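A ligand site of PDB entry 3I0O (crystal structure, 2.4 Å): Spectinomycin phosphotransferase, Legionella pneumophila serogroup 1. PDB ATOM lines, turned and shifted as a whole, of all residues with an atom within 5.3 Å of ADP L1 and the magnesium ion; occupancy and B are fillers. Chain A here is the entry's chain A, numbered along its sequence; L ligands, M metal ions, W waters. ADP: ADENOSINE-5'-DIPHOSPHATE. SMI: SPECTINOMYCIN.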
ATOM      1  N   GLY A  32     -16.971  -7.068  -4.431  1.00  0.00           N
ATOM      2  CA  GLY A  32     -15.909  -7.850  -3.801  1.00  0.00           C
ATOM      3  C   GLY A  32     -16.399  -8.975  -2.899  1.00  0.00           C
ATOM      4  O   GLY A  32     -17.337  -8.797  -2.127  1.00  0.00           O
ATOM      5  N   ALA A  33     -15.735 -10.130  -2.985  1.00  0.00           N
ATOM      6  CA  ALA A  33     -16.095 -11.291  -2.167  1.00  0.00           C
ATOM      7  C   ALA A  33     -15.982 -10.935  -0.688  1.00  0.00           C
ATOM      8  O   ALA A  33     -16.828 -11.319   0.123  1.00  0.00           O
ATOM      9  CB  ALA A  33     -15.183 -12.465  -2.494  1.00  0.00           C
ATOM     10  N   PHE A  50      -9.266  -6.741 -16.280  1.00  0.00           N
ATOM     11  CA  PHE A  50      -9.921  -6.928 -14.997  1.00  0.00           C
ATOM     12  C   PHE A  50      -8.835  -7.519 -14.108  1.00  0.00           C
ATOM     13  O   PHE A  50      -8.355  -8.619 -14.349  1.00  0.00           O
ATOM     14  CB  PHE A  50     -11.097  -7.885 -15.163  1.00  0.00           C
ATOM     15  CG  PHE A  50     -11.804  -8.214 -13.878  1.00  0.00           C
ATOM     16  CD1 PHE A  50     -11.459  -9.354 -13.151  1.00  0.00           C
ATOM     17  CD2 PHE A  50     -12.825  -7.401 -13.398  1.00  0.00           C
ATOM     18  CE1 PHE A  50     -12.124  -9.675 -11.972  1.00  0.00           C
ATOM     19  CE2 PHE A  50     -13.501  -7.704 -12.207  1.00  0.00           C
ATOM     20  CZ  PHE A  50     -13.145  -8.850 -11.501  1.00  0.00           C
ATOM     21  N   LYS A  52      -7.367  -8.747 -10.417  1.00  0.00           N
ATOM     22  CA  LYS A  52      -7.705  -9.298  -9.118  1.00  0.00           C
ATOM     23  C   LYS A  52      -6.463  -9.349  -8.234  1.00  0.00           C
ATOM     24  O   LYS A  52      -5.428  -9.852  -8.631  1.00  0.00           O
ATOM     25  CB  LYS A  52      -8.255 -10.711  -9.248  1.00  0.00           C
ATOM     26  CG  LYS A  52      -9.677 -10.812  -9.769  1.00  0.00           C
ATOM     27  CD  LYS A  52     -10.191 -12.260  -9.687  1.00  0.00           C
ATOM     28  CE  LYS A  52     -11.652 -12.364 -10.131  1.00  0.00           C
ATOM     29  NZ  LYS A  52     -12.202 -13.741  -9.981  1.00  0.00           N
ATOM     30  N   ILE A  78     -12.447 -17.429 -18.783  1.00  0.00           N
ATOM     31  CA  ILE A  78     -11.605 -16.284 -19.041  1.00  0.00           C
ATOM     32  C   ILE A  78     -10.169 -16.614 -18.672  1.00  0.00           C
ATOM     33  O   ILE A  78      -9.836 -16.692 -17.496  1.00  0.00           O
ATOM     34  CB  ILE A  78     -12.077 -15.054 -18.228  1.00  0.00           C
ATOM     35  CG1 ILE A  78     -13.596 -14.889 -18.399  1.00  0.00           C
ATOM     36  CG2 ILE A  78     -11.343 -13.816 -18.686  1.00  0.00           C
ATOM     37  CD1 ILE A  78     -14.207 -13.738 -17.604  1.00  0.00           C
ATOM     38  N   TYR A 100      -6.902 -10.333 -16.173  1.00  0.00           N
ATOM     39  CA  TYR A 100      -7.693 -11.007 -17.177  1.00  0.00           C
ATOM     40  C   TYR A 100      -8.163  -9.943 -18.134  1.00  0.00           C
ATOM     41  O   TYR A 100      -8.109  -8.769 -17.812  1.00  0.00           O
ATOM     42  CB  TYR A 100      -8.967 -11.650 -16.609  1.00  0.00           C
ATOM     43  CG  TYR A 100      -8.792 -12.677 -15.525  1.00  0.00           C
ATOM     44  CD1 TYR A 100      -8.633 -12.296 -14.191  1.00  0.00           C
ATOM     45  CD2 TYR A 100      -8.840 -14.037 -15.826  1.00  0.00           C
ATOM     46  CE1 TYR A 100      -8.528 -13.249 -13.194  1.00  0.00           C
ATOM     47  CE2 TYR A 100      -8.746 -15.001 -14.823  1.00  0.00           C
ATOM     48  CZ  TYR A 100      -8.584 -14.605 -13.516  1.00  0.00           C
ATOM     49  OH  TYR A 100      -8.499 -15.558 -12.522  1.00  0.00           O
ATOM     50  N   PRO A 101      -8.579 -10.318 -19.333  1.00  0.00           N
ATOM     51  CA  PRO A 101      -9.059  -9.249 -20.199  1.00  0.00           C
ATOM     52  C   PRO A 101     -10.404  -8.850 -19.558  1.00  0.00           C
ATOM     53  O   PRO A 101     -10.994  -9.647 -18.816  1.00  0.00           O
ATOM     54  CB  PRO A 101      -9.239  -9.942 -21.546  1.00  0.00           C
ATOM     55  CG  PRO A 101      -9.523 -11.374 -21.172  1.00  0.00           C
ATOM     56  CD  PRO A 101      -8.562 -11.621 -20.036  1.00  0.00           C
ATOM     57  N   PHE A 102     -10.888  -7.647 -19.821  1.00  0.00           N
ATOM     58  CA  PHE A 102     -12.146  -7.228 -19.238  1.00  0.00           C
ATOM     59  C   PHE A 102     -13.298  -7.649 -20.138  1.00  0.00           C
ATOM     60  O   PHE A 102     -13.275  -7.390 -21.347  1.00  0.00           O
ATOM     61  CB  PHE A 102     -12.173  -5.706 -19.061  1.00  0.00           C
ATOM     62  CG  PHE A 102     -13.248  -5.233 -18.123  1.00  0.00           C
ATOM     63  CD1 PHE A 102     -12.959  -4.993 -16.787  1.00  0.00           C
ATOM     64  CD2 PHE A 102     -14.555  -5.030 -18.571  1.00  0.00           C
ATOM     65  CE1 PHE A 102     -13.958  -4.551 -15.897  1.00  0.00           C
ATOM     66  CE2 PHE A 102     -15.552  -4.595 -17.702  1.00  0.00           C
ATOM     67  CZ  PHE A 102     -15.254  -4.355 -16.365  1.00  0.00           C
ATOM     68  N   ILE A 103     -14.294  -8.304 -19.541  1.00  0.00           N
ATOM     69  CA  ILE A 103     -15.487  -8.766 -20.259  1.00  0.00           C
ATOM     70  C   ILE A 103     -16.680  -7.905 -19.769  1.00  0.00           C
ATOM     71  O   ILE A 103     -17.001  -7.911 -18.582  1.00  0.00           O
ATOM     72  CB  ILE A 103     -15.764 -10.269 -19.946  1.00  0.00           C
ATOM     73  CG1 ILE A 103     -14.553 -11.118 -20.319  1.00  0.00           C
ATOM     74  CG2 ILE A 103     -17.016 -10.749 -20.683  1.00  0.00           C
ATOM     75  CD1 ILE A 103     -14.252 -11.167 -21.793  1.00  0.00           C
ATOM     76  N   HIS A 104     -17.320  -7.185 -20.680  1.00  0.00           N
ATOM     77  CA  HIS A 104     -18.439  -6.314 -20.313  1.00  0.00           C
ATOM     78  C   HIS A 104     -19.808  -6.973 -20.084  1.00  0.00           C
ATOM     79  O   HIS A 104     -20.718  -6.353 -19.531  1.00  0.00           O
ATOM     80  CB  HIS A 104     -18.578  -5.202 -21.358  1.00  0.00           C
ATOM     81  CG  HIS A 104     -17.468  -4.185 -21.312  1.00  0.00           C
ATOM     82  ND1 HIS A 104     -17.456  -3.144 -20.425  1.00  0.00           N
ATOM     83  CD2 HIS A 104     -16.314  -4.098 -22.017  1.00  0.00           C
ATOM     84  CE1 HIS A 104     -16.339  -2.451 -20.565  1.00  0.00           C
ATOM     85  NE2 HIS A 104     -15.625  -3.016 -21.527  1.00  0.00           N
ATOM     86  N   ASN A 107     -23.927 -10.506 -15.596  1.00  0.00           N
ATOM     87  CA  ASN A 107     -24.040 -11.872 -15.120  1.00  0.00           C
ATOM     88  C   ASN A 107     -25.461 -12.401 -15.324  1.00  0.00           C
ATOM     89  O   ASN A 107     -26.327 -11.681 -15.810  1.00  0.00           O
ATOM     90  CB  ASN A 107     -23.619 -11.978 -13.643  1.00  0.00           C
ATOM     91  CG  ASN A 107     -24.528 -11.207 -12.719  1.00  0.00           C
ATOM     92  OD1 ASN A 107     -25.747 -11.191 -12.892  1.00  0.00           O
ATOM     93  ND2 ASN A 107     -23.929 -10.565 -11.711  1.00  0.00           N
ATOM     94  N   ASP A 212     -20.090 -24.072  -7.592  1.00  0.00           N
ATOM     95  CA  ASP A 212     -20.845 -22.869  -7.314  1.00  0.00           C
ATOM     96  C   ASP A 212     -21.292 -22.195  -8.608  1.00  0.00           C
ATOM     97  O   ASP A 212     -21.239 -20.969  -8.726  1.00  0.00           O
ATOM     98  CB  ASP A 212     -19.965 -21.955  -6.464  1.00  0.00           C
ATOM     99  CG  ASP A 212     -20.709 -20.755  -5.920  1.00  0.00           C
ATOM    100  OD1 ASP A 212     -21.817 -20.927  -5.368  1.00  0.00           O
ATOM    101  OD2 ASP A 212     -20.146 -19.628  -6.019  1.00  0.00           O
ATOM    102  N   HIS A 214     -24.000 -20.945 -10.342  1.00  0.00           N
ATOM    103  CA  HIS A 214     -25.345 -20.418 -10.425  1.00  0.00           C
ATOM    104  C   HIS A 214     -25.246 -19.259 -11.426  1.00  0.00           C
ATOM    105  O   HIS A 214     -24.179 -19.008 -11.970  1.00  0.00           O
ATOM    106  CB  HIS A 214     -25.812 -19.926  -9.060  1.00  0.00           C
ATOM    107  CG  HIS A 214     -24.844 -19.027  -8.366  1.00  0.00           C
ATOM    108  ND1 HIS A 214     -24.698 -17.696  -8.691  1.00  0.00           N
ATOM    109  CD2 HIS A 214     -23.983 -19.258  -7.340  1.00  0.00           C
ATOM    110  CE1 HIS A 214     -23.784 -17.148  -7.898  1.00  0.00           C
ATOM    111  NE2 HIS A 214     -23.338 -18.069  -7.073  1.00  0.00           N
ATOM    112  N   GLY A 216     -25.060 -16.074 -11.063  1.00  0.00           N
ATOM    113  CA  GLY A 216     -24.139 -15.001 -10.754  1.00  0.00           C
ATOM    114  C   GLY A 216     -22.732 -15.314 -11.231  1.00  0.00           C
ATOM    115  O   GLY A 216     -21.903 -14.418 -11.389  1.00  0.00           O
ATOM    116  N   ASN A 217     -22.454 -16.589 -11.472  1.00  0.00           N
ATOM    117  CA  ASN A 217     -21.140 -16.979 -11.921  1.00  0.00           C
ATOM    118  C   ASN A 217     -21.093 -17.315 -13.388  1.00  0.00           C
ATOM    119  O   ASN A 217     -20.275 -18.114 -13.848  1.00  0.00           O
ATOM    120  CB  ASN A 217     -20.599 -18.127 -11.062  1.00  0.00           C
ATOM    121  CG  ASN A 217     -20.173 -17.660  -9.683  1.00  0.00           C
ATOM    122  OD1 ASN A 217     -19.615 -16.571  -9.554  1.00  0.00           O
ATOM    123  ND2 ASN A 217     -20.432 -18.468  -8.663  1.00  0.00           N
ATOM    124  N   LEU A 219     -21.276 -15.111 -17.082  1.00  0.00           N
ATOM    125  CA  LEU A 219     -21.312 -13.834 -17.763  1.00  0.00           C
ATOM    126  C   LEU A 219     -21.963 -14.137 -19.108  1.00  0.00           C
ATOM    127  O   LEU A 219     -21.462 -14.948 -19.880  1.00  0.00           O
ATOM    128  CB  LEU A 219     -19.909 -13.262 -17.951  1.00  0.00           C
ATOM    129  CG  LEU A 219     -19.264 -12.801 -16.642  1.00  0.00           C
ATOM    130  CD1 LEU A 219     -17.967 -12.040 -16.944  1.00  0.00           C
ATOM    131  CD2 LEU A 219     -20.247 -11.914 -15.870  1.00  0.00           C
ATOM    132  N   ILE A 229     -17.331 -18.096 -14.641  1.00  0.00           N
ATOM    133  CA  ILE A 229     -16.311 -17.473 -13.803  1.00  0.00           C
ATOM    134  C   ILE A 229     -16.318 -18.028 -12.397  1.00  0.00           C
ATOM    135  O   ILE A 229     -17.012 -18.995 -12.103  1.00  0.00           O
ATOM    136  CB  ILE A 229     -16.530 -15.959 -13.720  1.00  0.00           C
ATOM    137  CG1 ILE A 229     -17.943 -15.673 -13.197  1.00  0.00           C
ATOM    138  CG2 ILE A 229     -16.324 -15.336 -15.094  1.00  0.00           C
ATOM    139  CD1 ILE A 229     -18.219 -14.196 -12.954  1.00  0.00           C
ATOM    140  N   ASP A 230     -15.523 -17.392 -11.531  1.00  0.00           N
ATOM    141  CA  ASP A 230     -15.437 -17.783 -10.128  1.00  0.00           C
ATOM    142  C   ASP A 230     -14.932 -19.211  -9.982  1.00  0.00           C
ATOM    143  O   ASP A 230     -15.654 -20.095  -9.514  1.00  0.00           O
ATOM    144  CB  ASP A 230     -16.826 -17.651  -9.475  1.00  0.00           C
ATOM    145  CG  ASP A 230     -16.758 -17.157  -8.030  1.00  0.00           C
ATOM    146  OD1 ASP A 230     -15.668 -17.185  -7.425  1.00  0.00           O
ATOM    147  OD2 ASP A 230     -17.808 -16.727  -7.504  1.00  0.00           O
ATOM    148  N   ASP A 232     -12.880 -20.621  -7.867  1.00  0.00           N
ATOM    149  CA  ASP A 232     -12.164 -20.629  -6.597  1.00  0.00           C
ATOM    150  C   ASP A 232     -12.434 -21.880  -5.783  1.00  0.00           C
ATOM    151  O   ASP A 232     -11.634 -22.245  -4.929  1.00  0.00           O
ATOM    152  CB  ASP A 232     -12.517 -19.402  -5.760  1.00  0.00           C
ATOM    153  CG  ASP A 232     -12.054 -18.097  -6.401  1.00  0.00           C
ATOM    154  OD1 ASP A 232     -10.856 -17.993  -6.772  1.00  0.00           O
ATOM    155  OD2 ASP A 232     -12.889 -17.182  -6.526  1.00  0.00           O
HETATM  156  PB  ADP L   1     -16.279 -13.446  -6.345  1.00  0.00           P
HETATM  157  O1B ADP L   1     -15.893 -14.842  -6.023  1.00  0.00           O
HETATM  158  O2B ADP L   1     -15.835 -12.341  -5.451  1.00  0.00           O
HETATM  159  O3B ADP L   1     -17.894 -13.380  -6.472  1.00  0.00           O
HETATM  160  PA  ADP L   1     -16.379 -13.685  -9.220  1.00  0.00           P
HETATM  161  O1A ADP L   1     -15.288 -14.364  -9.956  1.00  0.00           O
HETATM  162  O2A ADP L   1     -17.632 -14.421  -8.950  1.00  0.00           O
HETATM  163  O3A ADP L   1     -15.762 -13.106  -7.833  1.00  0.00           O
HETATM  164  O5' ADP L   1     -16.766 -12.324 -10.007  1.00  0.00           O
HETATM  165  C5' ADP L   1     -17.723 -11.399  -9.460  1.00  0.00           C
HETATM  166  C4' ADP L   1     -18.136 -10.344 -10.484  1.00  0.00           C
HETATM  167  O4' ADP L   1     -16.985  -9.665 -11.030  1.00  0.00           O
HETATM  168  C3' ADP L   1     -18.859 -10.886 -11.734  1.00  0.00           C
HETATM  169  O3' ADP L   1     -20.279 -10.821 -11.534  1.00  0.00           O
HETATM  170  C2' ADP L   1     -18.453  -9.855 -12.804  1.00  0.00           C
HETATM  171  O2' ADP L   1     -19.347  -8.722 -12.726  1.00  0.00           O
HETATM  172  C1' ADP L   1     -17.030  -9.394 -12.438  1.00  0.00           C
HETATM  173  N9  ADP L   1     -15.950 -10.029 -13.259  1.00  0.00           N
HETATM  174  C8  ADP L   1     -15.278 -11.213 -13.044  1.00  0.00           C
HETATM  175  N7  ADP L   1     -14.387 -11.501 -13.951  1.00  0.00           N
HETATM  176  C5  ADP L   1     -14.462 -10.444 -14.845  1.00  0.00           C
HETATM  177  C6  ADP L   1     -13.762 -10.124 -16.071  1.00  0.00           C
HETATM  178  N6  ADP L   1     -12.827 -10.902 -16.586  1.00  0.00           N
HETATM  179  N1  ADP L   1     -14.095  -8.968 -16.713  1.00  0.00           N
HETATM  180  C2  ADP L   1     -15.051  -8.171 -16.197  1.00  0.00           C
HETATM  181  N3  ADP L   1     -15.768  -8.352 -15.073  1.00  0.00           N
HETATM  182  C4  ADP L   1     -15.415  -9.528 -14.432  1.00  0.00           C
HETATM  183  O1  SMI L   2     -24.673 -15.380  -4.330  1.00  0.00           O
HETATM  184  C2  SMI L   2     -25.791 -14.467  -4.160  1.00  0.00           C
HETATM  185  C2M SMI L   2     -25.315 -13.055  -4.456  1.00  0.00           C
HETATM  186  C3  SMI L   2     -26.355 -14.571  -2.690  1.00  0.00           C
HETATM  187  C4  SMI L   2     -26.769 -16.014  -2.505  1.00  0.00           C
HETATM  188  C5  SMI L   2     -25.463 -16.781  -2.630  1.00  0.00           C
HETATM  189  O5  SMI L   2     -25.809 -18.158  -2.416  1.00  0.00           O
HETATM  190  C6  SMI L   2     -25.025 -16.764  -4.067  1.00  0.00           C
HETATM  191  O1B SMI L   2     -24.478 -16.411  -1.675  1.00  0.00           O
HETATM  192  O2B SMI L   2     -23.748 -17.385  -4.283  1.00  0.00           O
HETATM  193  C7  SMI L   2     -23.338 -17.231  -1.857  1.00  0.00           C
HETATM  194  C8  SMI L   2     -22.294 -16.858  -0.793  1.00  0.00           C
HETATM  195  N8  SMI L   2     -22.943 -17.081   0.526  1.00  0.00           N
HETATM  196  C8M SMI L   2     -22.034 -16.734   1.621  1.00  0.00           C
HETATM  197  C9  SMI L   2     -21.055 -17.799  -0.975  1.00  0.00           C
HETATM  198  O9  SMI L   2     -21.475 -19.166  -0.819  1.00  0.00           O
HETATM  199  C10 SMI L   2     -20.464 -17.609  -2.407  1.00  0.00           C
HETATM  200  N10 SMI L   2     -19.400 -18.443  -2.631  1.00  0.00           N
HETATM  201  C1M SMI L   2     -18.272 -18.229  -1.707  1.00  0.00           C
HETATM  202  C11 SMI L   2     -21.541 -17.916  -3.444  1.00  0.00           C
HETATM  203  O11 SMI L   2     -20.996 -17.720  -4.728  1.00  0.00           O
HETATM  204  C12 SMI L   2     -22.760 -17.025  -3.268  1.00  0.00           C
HETATM  205  O4A SMI L   2     -27.352 -16.308  -1.241  1.00  0.00           O
HETATM  206  O4B SMI L   2     -27.740 -16.059  -3.466  1.00  0.00           O
HETATM  207 MG    MG M   1     -19.148 -15.071  -7.920  1.00  0.00          MG
HETATM  208  O   HOH W   1     -15.762 -17.178  -4.814  1.00  0.00           O
HETATM  209  O   HOH W   2     -20.349 -14.063  -8.824  1.00  0.00           O
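The backbone NH (N) of Asp 230 is in hydrogen-bond range of an oxygen (O1A) of ADP L1 (3.4 Å).
N1 of ADP L1 lies within hydrogen-bond range of N of Ile 103 (2.9 Å).
The backbone NH (N) of Ala 33 lies close to an oxygen (O2B) of ADP L1 (3.3 Å).
An oxygen (O1A) of ADP L1 is in salt-bridge range of the side-chain amino group (NZ) of Lys 52, at 3.1 Å.
O of Pro 101 is in hydrogen-bond range of N6 of ADP L1 (3.1 Å).
A nitrogen (N10) of SMI L2 lies within salt-bridge range of the side-chain carboxylate (OD2) of Asp 212 (3.7 Å).
NE2 of His 214 sits at hydrogen-bond distance from O2B of SMI L2.
The backbone carbonyl oxygen (O) of Asn 217 lies within hydrogen-bond range of the backbone NH (N) of Ile 229 (3.0 Å).
ND2 of Asn 217 is in hydrogen-bond range of O of Asp 212, 2.6 Å away.
The side-chain amide nitrogen of Asn 217 lies within hydrogen-bond range of a ring nitrogen (NE2) of His 214 (3.3 Å).
N of Phe 50 is in hydrogen-bond range of O of Tyr 100 (2.8 Å).
The backbone NH of Gly 216 lies within hydrogen-bond range of a ring nitrogen (ND1) of His 214, at 2.9 Å.
CE2 of Phe 50 touches C4 of ADP L1, 3.5 Å away.
Ile 78 touches ADP L1 (CD1 to N6, 3.3 Å).
Tyr 100 touches ADP L1.
Phe 102 touches ADP L1 (CA to N1, 3.6 Å).
ND2 of Asn 107 touches O3' of ADP L1 (3.7 Å).
Gly 216 touches ADP L1 (O to O3', 3.9 Å).
Ile 229 touches ADP L1 (CD1 to C3', 3.6 Å).
OD2 of Asp 232 touches O1B of ADP L1, at 3.8 Å.
Hydrophobic or aromatic side chains that line ADP L1: Ala 33, Phe 50, Ile 78, Tyr 100, Phe 102, Ile 103 and Ile 229.
The nearest printed residue that does not touch ADP L1 is Leu 219 (4.1 Å).
Of the 19 residues printed, 2 come within 4 Å of the magnesium ion.
The nearest printed residue that does not touch the magnesium ion is Gly 216 (4.5 Å).
The magnesium ion is bound by water W2 (1.8 Å), an oxygen (O2A) of ADP L1 (1.9 Å), the side-chain carboxylate of Asp 230 (2.2 Å), the side-chain amide oxygen of Asn 217 (2.3 Å) and an oxygen (O3B) of ADP L1 (2.6 Å).
Water W1 lies within hydrogen-bond range of OD1 of Asp 230 (2.6 Å), O1B of ADP L1 (2.6 Å) and OD2 of Asp 232 (3.3 Å).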
